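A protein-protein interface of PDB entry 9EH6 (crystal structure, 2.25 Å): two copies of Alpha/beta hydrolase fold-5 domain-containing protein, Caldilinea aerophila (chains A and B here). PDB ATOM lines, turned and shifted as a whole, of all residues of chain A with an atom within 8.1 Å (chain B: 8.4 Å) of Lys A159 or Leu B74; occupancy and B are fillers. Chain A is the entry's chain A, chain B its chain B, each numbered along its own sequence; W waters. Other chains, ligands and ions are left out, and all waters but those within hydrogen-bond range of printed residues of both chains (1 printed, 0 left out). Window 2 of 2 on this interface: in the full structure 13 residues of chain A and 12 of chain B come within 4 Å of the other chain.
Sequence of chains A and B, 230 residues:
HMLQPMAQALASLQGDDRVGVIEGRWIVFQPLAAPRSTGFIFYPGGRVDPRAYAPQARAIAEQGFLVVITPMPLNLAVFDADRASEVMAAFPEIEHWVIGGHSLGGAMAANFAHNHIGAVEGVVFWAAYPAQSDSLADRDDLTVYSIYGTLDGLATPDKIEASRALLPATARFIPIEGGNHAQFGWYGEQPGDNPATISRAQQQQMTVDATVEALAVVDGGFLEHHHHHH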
ATOM      1  N   ALA A 128      30.976  25.068 -14.771  1.00  0.00           N
ATOM      2  CA  ALA A 128      30.111  23.991 -14.305  1.00  0.00           C
ATOM      3  C   ALA A 128      29.064  24.514 -13.333  1.00  0.00           C
ATOM      4  O   ALA A 128      29.060  25.684 -12.980  1.00  0.00           O
ATOM      5  CB  ALA A 128      30.930  22.861 -13.727  1.00  0.00           C
ATOM      6  N   TYR A 129      28.154  23.628 -12.929  1.00  0.00           N
ATOM      7  CA  TYR A 129      27.031  23.939 -12.061  1.00  0.00           C
ATOM      8  C   TYR A 129      26.488  22.599 -11.573  1.00  0.00           C
ATOM      9  O   TYR A 129      26.787  21.567 -12.166  1.00  0.00           O
ATOM     10  CB  TYR A 129      26.034  24.858 -12.775  1.00  0.00           C
ATOM     11  CG  TYR A 129      25.566  24.378 -14.143  1.00  0.00           C
ATOM     12  CD1 TYR A 129      24.546  23.435 -14.263  1.00  0.00           C
ATOM     13  CD2 TYR A 129      26.151  24.842 -15.317  1.00  0.00           C
ATOM     14  CE1 TYR A 129      24.102  22.991 -15.500  1.00  0.00           C
ATOM     15  CE2 TYR A 129      25.728  24.392 -16.565  1.00  0.00           C
ATOM     16  CZ  TYR A 129      24.692  23.472 -16.661  1.00  0.00           C
ATOM     17  OH  TYR A 129      24.253  22.996 -17.871  1.00  0.00           O
ATOM     18  N   PRO A 130      25.780  22.539 -10.424  1.00  0.00           N
ATOM     19  CA  PRO A 130      25.238  21.273  -9.936  1.00  0.00           C
ATOM     20  C   PRO A 130      23.997  20.908 -10.742  1.00  0.00           C
ATOM     21  O   PRO A 130      23.337  21.780 -11.316  1.00  0.00           O
ATOM     22  CB  PRO A 130      24.760  21.584  -8.513  1.00  0.00           C
ATOM     23  CG  PRO A 130      25.333  22.956  -8.200  1.00  0.00           C
ATOM     24  CD  PRO A 130      25.500  23.668  -9.526  1.00  0.00           C
ATOM     25  N   ALA A 131      23.706  19.609 -10.773  1.00  0.00           N
ATOM     26  CA  ALA A 131      22.380  19.120 -11.114  1.00  0.00           C
ATOM     27  C   ALA A 131      21.402  19.602 -10.043  1.00  0.00           C
ATOM     28  O   ALA A 131      21.772  19.795  -8.882  1.00  0.00           O
ATOM     29  CB  ALA A 131      22.390  17.601 -11.205  1.00  0.00           C
ATOM     30  N   GLN A 132      20.157  19.784 -10.470  1.00  0.00           N
ATOM     31  CA  GLN A 132      19.012  20.032  -9.615  1.00  0.00           C
ATOM     32  C   GLN A 132      19.043  19.173  -8.351  1.00  0.00           C
ATOM     33  O   GLN A 132      18.902  19.677  -7.238  1.00  0.00           O
ATOM     34  CB  GLN A 132      17.770  19.786 -10.471  1.00  0.00           C
ATOM     35  CG  GLN A 132      17.168  21.066 -11.028  1.00  0.00           C
ATOM     36  CD  GLN A 132      16.351  21.820 -10.001  1.00  0.00           C
ATOM     37  OE1 GLN A 132      16.499  21.653  -8.787  1.00  0.00           O
ATOM     38  NE2 GLN A 132      15.461  22.661 -10.499  1.00  0.00           N
ATOM     39  N   SER A 146      32.225  30.162  -8.704  1.00  0.00           N
ATOM     40  CA  SER A 146      31.842  29.628  -9.992  1.00  0.00           C
ATOM     41  C   SER A 146      32.507  30.462 -11.089  1.00  0.00           C
ATOM     42  O   SER A 146      32.209  31.647 -11.283  1.00  0.00           O
ATOM     43  CB  SER A 146      30.332  29.578 -10.109  1.00  0.00           C
ATOM     44  OG  SER A 146      29.960  29.048 -11.377  1.00  0.00           O
ATOM     45  N   TYR A 148      33.642  31.121 -14.951  1.00  0.00           N
ATOM     46  CA  TYR A 148      32.984  30.756 -16.196  1.00  0.00           C
ATOM     47  C   TYR A 148      33.485  31.661 -17.314  1.00  0.00           C
ATOM     48  O   TYR A 148      33.842  32.814 -17.070  1.00  0.00           O
ATOM     49  CB  TYR A 148      31.450  30.759 -16.107  1.00  0.00           C
ATOM     50  CG  TYR A 148      30.835  32.142 -15.907  1.00  0.00           C
ATOM     51  CD1 TYR A 148      30.777  32.743 -14.643  1.00  0.00           C
ATOM     52  CD2 TYR A 148      30.336  32.859 -16.986  1.00  0.00           C
ATOM     53  CE1 TYR A 148      30.245  34.016 -14.464  1.00  0.00           C
ATOM     54  CE2 TYR A 148      29.785  34.121 -16.822  1.00  0.00           C
ATOM     55  CZ  TYR A 148      29.751  34.706 -15.565  1.00  0.00           C
ATOM     56  OH  TYR A 148      29.218  35.952 -15.446  1.00  0.00           O
ATOM     57  N   ASP A 152      31.658  30.614 -23.542  1.00  0.00           N
ATOM     58  CA  ASP A 152      31.530  29.172 -23.406  1.00  0.00           C
ATOM     59  C   ASP A 152      30.280  28.681 -24.151  1.00  0.00           C
ATOM     60  O   ASP A 152      29.173  29.134 -23.880  1.00  0.00           O
ATOM     61  CB  ASP A 152      31.618  28.764 -21.929  1.00  0.00           C
ATOM     62  CG  ASP A 152      31.482  27.272 -21.663  1.00  0.00           C
ATOM     63  OD1 ASP A 152      30.918  26.576 -22.527  1.00  0.00           O
ATOM     64  OD2 ASP A 152      31.966  26.809 -20.588  1.00  0.00           O
ATOM     65  N   LEU A 154      29.109  25.452 -24.256  1.00  0.00           N
ATOM     66  CA  LEU A 154      28.441  24.287 -23.669  1.00  0.00           C
ATOM     67  C   LEU A 154      27.719  24.692 -22.391  1.00  0.00           C
ATOM     68  O   LEU A 154      26.524  24.482 -22.262  1.00  0.00           O
ATOM     69  CB  LEU A 154      29.453  23.186 -23.354  1.00  0.00           C
ATOM     70  CG  LEU A 154      29.795  22.246 -24.504  1.00  0.00           C
ATOM     71  CD1 LEU A 154      30.563  22.988 -25.581  1.00  0.00           C
ATOM     72  CD2 LEU A 154      30.624  21.074 -23.990  1.00  0.00           C
ATOM     73  N   ALA A 155      28.457  25.282 -21.450  1.00  0.00           N
ATOM     74  CA  ALA A 155      27.851  25.836 -20.259  1.00  0.00           C
ATOM     75  C   ALA A 155      27.839  27.353 -20.426  1.00  0.00           C
ATOM     76  O   ALA A 155      28.830  28.005 -20.082  1.00  0.00           O
ATOM     77  CB  ALA A 155      28.680  25.404 -19.079  1.00  0.00           C
ATOM     78  N   THR A 156      26.765  27.883 -21.032  1.00  0.00           N
ATOM     79  CA  THR A 156      26.694  29.285 -21.443  1.00  0.00           C
ATOM     80  C   THR A 156      26.491  30.190 -20.226  1.00  0.00           C
ATOM     81  O   THR A 156      26.056  29.727 -19.174  1.00  0.00           O
ATOM     82  CB  THR A 156      25.523  29.572 -22.410  1.00  0.00           C
ATOM     83  OG1 THR A 156      24.298  29.193 -21.771  1.00  0.00           O
ATOM     84  CG2 THR A 156      25.673  28.951 -23.789  1.00  0.00           C
ATOM     85  N   PRO A 157      26.811  31.505 -20.309  1.00  0.00           N
ATOM     86  CA  PRO A 157      26.553  32.430 -19.203  1.00  0.00           C
ATOM     87  C   PRO A 157      25.125  32.371 -18.666  1.00  0.00           C
ATOM     88  O   PRO A 157      24.940  32.409 -17.446  1.00  0.00           O
ATOM     89  CB  PRO A 157      26.906  33.804 -19.794  1.00  0.00           C
ATOM     90  CG  PRO A 157      27.980  33.472 -20.814  1.00  0.00           C
ATOM     91  CD  PRO A 157      27.521  32.162 -21.422  1.00  0.00           C
ATOM     92  N   ASP A 158      24.131  32.255 -19.575  1.00  0.00           N
ATOM     93  CA  ASP A 158      22.734  32.203 -19.158  1.00  0.00           C
ATOM     94  C   ASP A 158      22.513  30.987 -18.257  1.00  0.00           C
ATOM     95  O   ASP A 158      21.882  31.077 -17.209  1.00  0.00           O
ATOM     96  CB  ASP A 158      21.755  32.332 -20.335  1.00  0.00           C
ATOM     97  CG  ASP A 158      21.734  33.694 -21.041  1.00  0.00           C
ATOM     98  OD1 ASP A 158      22.584  34.554 -20.736  1.00  0.00           O
ATOM     99  OD2 ASP A 158      20.874  33.888 -21.925  1.00  0.00           O
ATOM    100  N   LYS A 159      23.073  29.847 -18.650  1.00  0.00           N
ATOM    101  CA  LYS A 159      22.948  28.619 -17.884  1.00  0.00           C
ATOM    102  C   LYS A 159      23.646  28.734 -16.518  1.00  0.00           C
ATOM    103  O   LYS A 159      23.131  28.251 -15.512  1.00  0.00           O
ATOM    104  CB  LYS A 159      23.490  27.468 -18.742  1.00  0.00           C
ATOM    105  CG  LYS A 159      22.931  26.083 -18.441  1.00  0.00           C
ATOM    106  CD  LYS A 159      21.504  25.840 -18.894  1.00  0.00           C
ATOM    107  CE  LYS A 159      21.085  24.400 -18.643  1.00  0.00           C
ATOM    108  NZ  LYS A 159      19.637  24.149 -18.866  1.00  0.00           N
ATOM    109  N   ILE A 160      24.827  29.372 -16.471  1.00  0.00           N
ATOM    110  CA  ILE A 160      25.609  29.481 -15.241  1.00  0.00           C
ATOM    111  C   ILE A 160      24.861  30.351 -14.228  1.00  0.00           C
ATOM    112  O   ILE A 160      24.753  30.002 -13.049  1.00  0.00           O
ATOM    113  CB  ILE A 160      27.014  30.052 -15.537  1.00  0.00           C
ATOM    114  CG1 ILE A 160      27.844  29.110 -16.421  1.00  0.00           C
ATOM    115  CG2 ILE A 160      27.749  30.413 -14.252  1.00  0.00           C
ATOM    116  CD1 ILE A 160      28.553  27.996 -15.659  1.00  0.00           C
ATOM    117  N   GLU A 161      24.342  31.485 -14.720  1.00  0.00           N
ATOM    118  CA  GLU A 161      23.576  32.423 -13.912  1.00  0.00           C
ATOM    119  C   GLU A 161      22.340  31.738 -13.326  1.00  0.00           C
ATOM    120  O   GLU A 161      21.975  32.006 -12.178  1.00  0.00           O
ATOM    121  CB  GLU A 161      23.266  33.712 -14.692  1.00  0.00           C
ATOM    122  CG  GLU A 161      24.513  34.513 -15.010  1.00  0.00           C
ATOM    123  CD  GLU A 161      25.318  34.956 -13.797  1.00  0.00           C
ATOM    124  OE1 GLU A 161      24.736  34.927 -12.666  1.00  0.00           O
ATOM    125  OE2 GLU A 161      26.537  35.271 -13.953  1.00  0.00           O
ATOM    126  N   ALA A 162      21.714  30.832 -14.092  1.00  0.00           N
ATOM    127  CA  ALA A 162      20.539  30.136 -13.574  1.00  0.00           C
ATOM    128  C   ALA A 162      20.927  29.240 -12.399  1.00  0.00           C
ATOM    129  O   ALA A 162      20.118  29.018 -11.507  1.00  0.00           O
ATOM    130  CB  ALA A 162      19.769  29.390 -14.649  1.00  0.00           C
ATOM    131  N   SER A 163      22.192  28.815 -12.340  1.00  0.00           N
ATOM    132  CA  SER A 163      22.600  27.930 -11.252  1.00  0.00           C
ATOM    133  C   SER A 163      22.721  28.670  -9.917  1.00  0.00           C
ATOM    134  O   SER A 163      22.962  28.029  -8.901  1.00  0.00           O
ATOM    135  CB  SER A 163      23.848  27.149 -11.580  1.00  0.00           C
ATOM    136  OG  SER A 163      25.013  27.938 -11.387  1.00  0.00           O
ATOM    137  N   ARG A 164      22.524  30.003  -9.900  1.00  0.00           N
ATOM    138  CA  ARG A 164      22.467  30.700  -8.616  1.00  0.00           C
ATOM    139  C   ARG A 164      21.451  30.054  -7.679  1.00  0.00           C
ATOM    140  O   ARG A 164      21.725  29.911  -6.500  1.00  0.00           O
ATOM    141  CB  ARG A 164      22.288  32.215  -8.735  1.00  0.00           C
ATOM    142  CG  ARG A 164      23.544  32.938  -9.221  1.00  0.00           C
ATOM    143  CD  ARG A 164      23.194  34.391  -9.545  1.00  0.00           C
ATOM    144  NE  ARG A 164      24.310  35.245  -9.915  1.00  0.00           N
ATOM    145  CZ  ARG A 164      25.163  35.816  -9.061  1.00  0.00           C
ATOM    146  NH1 ARG A 164      25.040  35.633  -7.761  1.00  0.00           N
ATOM    147  NH2 ARG A 164      26.139  36.587  -9.513  1.00  0.00           N
ATOM    148  N   ALA A 165      20.310  29.611  -8.203  1.00  0.00           N
ATOM    149  CA  ALA A 165      19.279  29.008  -7.377  1.00  0.00           C
ATOM    150  C   ALA A 165      19.759  27.725  -6.692  1.00  0.00           C
ATOM    151  O   ALA A 165      19.120  27.302  -5.728  1.00  0.00           O
ATOM    152  CB  ALA A 165      18.066  28.712  -8.230  1.00  0.00           C
ATOM    153  N   LEU A 166      20.862  27.113  -7.185  1.00  0.00           N
ATOM    154  CA  LEU A 166      21.349  25.829  -6.679  1.00  0.00           C
ATOM    155  C   LEU A 166      22.605  26.010  -5.838  1.00  0.00           C
ATOM    156  O   LEU A 166      23.277  25.032  -5.506  1.00  0.00           O
ATOM    157  CB  LEU A 166      21.618  24.880  -7.854  1.00  0.00           C
ATOM    158  CG  LEU A 166      20.372  24.500  -8.659  1.00  0.00           C
ATOM    159  CD1 LEU A 166      20.721  23.638  -9.864  1.00  0.00           C
ATOM    160  CD2 LEU A 166      19.337  23.801  -7.772  1.00  0.00           C
ATOM    161  N   PHE A 173      30.454  34.458  -8.346  1.00  0.00           N
ATOM    162  CA  PHE A 173      30.557  34.154  -9.763  1.00  0.00           C
ATOM    163  C   PHE A 173      31.680  34.988 -10.356  1.00  0.00           C
ATOM    164  O   PHE A 173      31.707  36.202 -10.157  1.00  0.00           O
ATOM    165  CB  PHE A 173      29.204  34.362 -10.452  1.00  0.00           C
ATOM    166  CG  PHE A 173      28.240  33.250 -10.137  1.00  0.00           C
ATOM    167  CD1 PHE A 173      27.728  33.096  -8.857  1.00  0.00           C
ATOM    168  CD2 PHE A 173      27.904  32.313 -11.105  1.00  0.00           C
ATOM    169  CE1 PHE A 173      26.872  32.049  -8.554  1.00  0.00           C
ATOM    170  CE2 PHE A 173      27.023  31.278 -10.808  1.00  0.00           C
ATOM    171  CZ  PHE A 173      26.527  31.141  -9.531  1.00  0.00           C
ATOM    172  N   ARG B  25       9.570  16.803 -23.699  1.00  0.00           N
ATOM    173  CA  ARG B  25      11.002  16.984 -23.519  1.00  0.00           C
ATOM    174  C   ARG B  25      11.628  17.217 -24.903  1.00  0.00           C
ATOM    175  O   ARG B  25      12.660  17.866 -25.038  1.00  0.00           O
ATOM    176  CB  ARG B  25      11.597  15.760 -22.810  1.00  0.00           C
ATOM    177  CG  ARG B  25      11.721  14.541 -23.718  1.00  0.00           C
ATOM    178  CD  ARG B  25      11.939  13.215 -22.998  1.00  0.00           C
ATOM    179  NE  ARG B  25      13.298  13.141 -22.455  1.00  0.00           N
ATOM    180  CZ  ARG B  25      13.888  12.047 -21.988  1.00  0.00           C
ATOM    181  NH1 ARG B  25      13.241  10.893 -21.947  1.00  0.00           N
ATOM    182  NH2 ARG B  25      15.135  12.116 -21.554  1.00  0.00           N
ATOM    183  N   PRO B  71      16.295  19.398 -27.710  1.00  0.00           N
ATOM    184  CA  PRO B  71      16.935  20.537 -27.045  1.00  0.00           C
ATOM    185  C   PRO B  71      18.205  20.165 -26.296  1.00  0.00           C
ATOM    186  O   PRO B  71      18.428  18.993 -25.997  1.00  0.00           O
ATOM    187  CB  PRO B  71      15.899  21.063 -26.037  1.00  0.00           C
ATOM    188  CG  PRO B  71      14.579  20.501 -26.529  1.00  0.00           C
ATOM    189  CD  PRO B  71      14.894  19.224 -27.300  1.00  0.00           C
ATOM    190  N   MET B  72      19.031  21.189 -26.038  1.00  0.00           N
ATOM    191  CA  MET B  72      20.260  21.023 -25.290  1.00  0.00           C
ATOM    192  C   MET B  72      19.917  20.503 -23.905  1.00  0.00           C
ATOM    193  O   MET B  72      18.888  20.863 -23.344  1.00  0.00           O
ATOM    194  CB  MET B  72      21.055  22.329 -25.184  1.00  0.00           C
ATOM    195  CG  MET B  72      22.453  22.218 -25.800  1.00  0.00           C
ATOM    196  SD  MET B  72      22.974  23.732 -26.640  1.00  0.00           S
ATOM    197  CE  MET B  72      21.455  24.192 -27.484  1.00  0.00           C
ATOM    198  N   PRO B  73      20.762  19.616 -23.339  1.00  0.00           N
ATOM    199  CA  PRO B  73      20.559  19.117 -21.977  1.00  0.00           C
ATOM    200  C   PRO B  73      20.344  20.220 -20.934  1.00  0.00           C
ATOM    201  O   PRO B  73      20.887  21.324 -21.037  1.00  0.00           O
ATOM    202  CB  PRO B  73      21.866  18.348 -21.695  1.00  0.00           C
ATOM    203  CG  PRO B  73      22.848  18.788 -22.770  1.00  0.00           C
ATOM    204  CD  PRO B  73      21.974  19.071 -23.971  1.00  0.00           C
ATOM    205  N   LEU B  74      19.541  19.895 -19.920  1.00  0.00           N
ATOM    206  CA  LEU B  74      19.344  20.756 -18.765  1.00  0.00           C
ATOM    207  C   LEU B  74      20.593  20.703 -17.880  1.00  0.00           C
ATOM    208  O   LEU B  74      20.982  21.718 -17.304  1.00  0.00           O
ATOM    209  CB  LEU B  74      18.109  20.246 -18.016  1.00  0.00           C
ATOM    210  CG  LEU B  74      16.811  20.245 -18.823  1.00  0.00           C
ATOM    211  CD1 LEU B  74      15.979  19.014 -18.497  1.00  0.00           C
ATOM    212  CD2 LEU B  74      16.009  21.518 -18.562  1.00  0.00           C
ATOM    213  N   ASN B  75      21.208  19.509 -17.798  1.00  0.00           N
ATOM    214  CA  ASN B  75      22.316  19.196 -16.903  1.00  0.00           C
ATOM    215  C   ASN B  75      23.501  18.625 -17.683  1.00  0.00           C
ATOM    216  O   ASN B  75      23.337  18.141 -18.803  1.00  0.00           O
ATOM    217  CB  ASN B  75      21.896  18.244 -15.777  1.00  0.00           C
ATOM    218  CG  ASN B  75      21.116  18.941 -14.679  1.00  0.00           C
ATOM    219  OD1 ASN B  75      20.105  18.423 -14.206  1.00  0.00           O
ATOM    220  ND2 ASN B  75      21.597  20.096 -14.242  1.00  0.00           N
ATOM    221  N   LEU B  76      24.689  18.668 -17.063  1.00  0.00           N
ATOM    222  CA  LEU B  76      25.936  18.304 -17.720  1.00  0.00           C
ATOM    223  C   LEU B  76      26.161  16.793 -17.729  1.00  0.00           C
ATOM    224  O   LEU B  76      26.945  16.321 -18.546  1.00  0.00           O
ATOM    225  CB  LEU B  76      27.110  19.051 -17.077  1.00  0.00           C
ATOM    226  CG  LEU B  76      27.284  20.508 -17.513  1.00  0.00           C
ATOM    227  CD1 LEU B  76      28.196  21.269 -16.551  1.00  0.00           C
ATOM    228  CD2 LEU B  76      27.821  20.597 -18.936  1.00  0.00           C
ATOM    229  N   ALA B  77      25.459  16.040 -16.863  1.00  0.00           N
ATOM    230  CA  ALA B  77      25.492  14.579 -16.902  1.00  0.00           C
ATOM    231  C   ALA B  77      24.856  14.062 -18.199  1.00  0.00           C
ATOM    232  O   ALA B  77      25.067  12.916 -18.603  1.00  0.00           O
ATOM    233  CB  ALA B  77      24.821  13.995 -15.682  1.00  0.00           C
ATOM    234  N   VAL B  78      24.076  14.931 -18.854  1.00  0.00           N
ATOM    235  CA  VAL B  78      23.427  14.599 -20.110  1.00  0.00           C
ATOM    236  C   VAL B  78      24.350  15.025 -21.257  1.00  0.00           C
ATOM    237  O   VAL B  78      23.962  15.758 -22.169  1.00  0.00           O
ATOM    238  CB  VAL B  78      21.990  15.168 -20.210  1.00  0.00           C
ATOM    239  CG1 VAL B  78      21.230  14.661 -21.436  1.00  0.00           C
ATOM    240  CG2 VAL B  78      21.180  14.916 -18.940  1.00  0.00           C
ATOM    241  N   PHE B  79      25.604  14.561 -21.181  1.00  0.00           N
ATOM    242  CA  PHE B  79      26.365  14.326 -22.395  1.00  0.00           C
ATOM    243  C   PHE B  79      25.716  13.155 -23.127  1.00  0.00           C
ATOM    244  O   PHE B  79      25.771  13.114 -24.350  1.00  0.00           O
ATOM    245  CB  PHE B  79      27.854  14.074 -22.117  1.00  0.00           C
ATOM    246  CG  PHE B  79      28.679  13.736 -23.338  1.00  0.00           C
ATOM    247  CD1 PHE B  79      29.262  12.481 -23.479  1.00  0.00           C
ATOM    248  CD2 PHE B  79      28.879  14.668 -24.351  1.00  0.00           C
ATOM    249  CE1 PHE B  79      30.013  12.167 -24.603  1.00  0.00           C
ATOM    250  CE2 PHE B  79      29.637  14.353 -25.472  1.00  0.00           C
ATOM    251  CZ  PHE B  79      30.202  13.103 -25.598  1.00  0.00           C
ATOM    252  N   ARG B  83      22.097  13.176 -25.861  1.00  0.00           N
ATOM    253  CA  ARG B  83      20.669  13.282 -25.644  1.00  0.00           C
ATOM    254  C   ARG B  83      19.944  12.515 -26.754  1.00  0.00           C
ATOM    255  O   ARG B  83      18.745  12.286 -26.689  1.00  0.00           O
ATOM    256  CB  ARG B  83      20.342  14.777 -25.588  1.00  0.00           C
ATOM    257  CG  ARG B  83      20.494  15.507 -26.912  1.00  0.00           C
ATOM    258  CD  ARG B  83      21.415  16.714 -26.862  1.00  0.00           C
ATOM    259  NE  ARG B  83      20.904  17.806 -27.669  1.00  0.00           N
ATOM    260  CZ  ARG B  83      21.595  18.867 -28.089  1.00  0.00           C
ATOM    261  NH1 ARG B  83      20.943  19.890 -28.613  1.00  0.00           N
ATOM    262  NH2 ARG B  83      22.911  18.925 -27.962  1.00  0.00           N
HETATM  263  O   HOH W   1      25.049  20.127 -14.110  1.00  0.00           O
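Water W1 lies within hydrogen-bond range of the backbone carbonyl oxygen (O) of Tyr A129 (3.0 Å), the backbone NH (N) of Leu B76 (3.3 Å) and the side-chain amide nitrogen (ND2) of Asn B75 (3.5 Å).
Among the printed residues, merely in contact across the chains: Tyr A129 with Leu B74, Tyr A129 with Leu B76, Pro A130 with Asn B75, Ala A131 with Asn B75, Gln A132 with Asn B75 and Lys A159 with Pro B73.
The side-chain amino group (NZ) of Lys A159 lies close to the backbone carbonyl oxygen (O) of Leu B74 (3.2 Å).
Of the 11 printed residues of chain B, 4 touch a printed residue of chain A.
Hydrophobic or aromatic side chains of chain B within 4 Å of the printed part of chain A: Leu B76.
Hydrophobic or aromatic side chains of chain A that line the printed part of chain B: Tyr A129 and Ala A131.
Among the printed residues, no Asp or Glu carboxylate lies within 4 Å of a Lys or Arg side-chain nitrogen of the other chain.
The side-chain hydroxyl of Thr A156 sits at hydrogen-bond distance from the backbone NH of Lys A159 (3.4 Å).
No position is printed for both chains.
Of the 7 pairs that touch across the chains among the printed residues, none has its exchanged pair printed and touching as well.
Lys A159 touches just these residues of chain B: Pro B73 (3.8 Å) and Leu B74 (3.0 Å).
Of the printed residues of chain A, Pro B73 touches Lys A159.
Of the printed residues of chain A, Asn B75 touches Pro A130, Ala A131 and Gln A132.
Of the printed residues of chain B, Ala A131 touches Asn B75 (3.4 Å).
The nearest residue of chain B that does not touch Lys A159 is Asn B75 (5.0 Å).
The nearest residue of chain A that does not touch Leu B74 is Pro A130 (6.4 Å).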
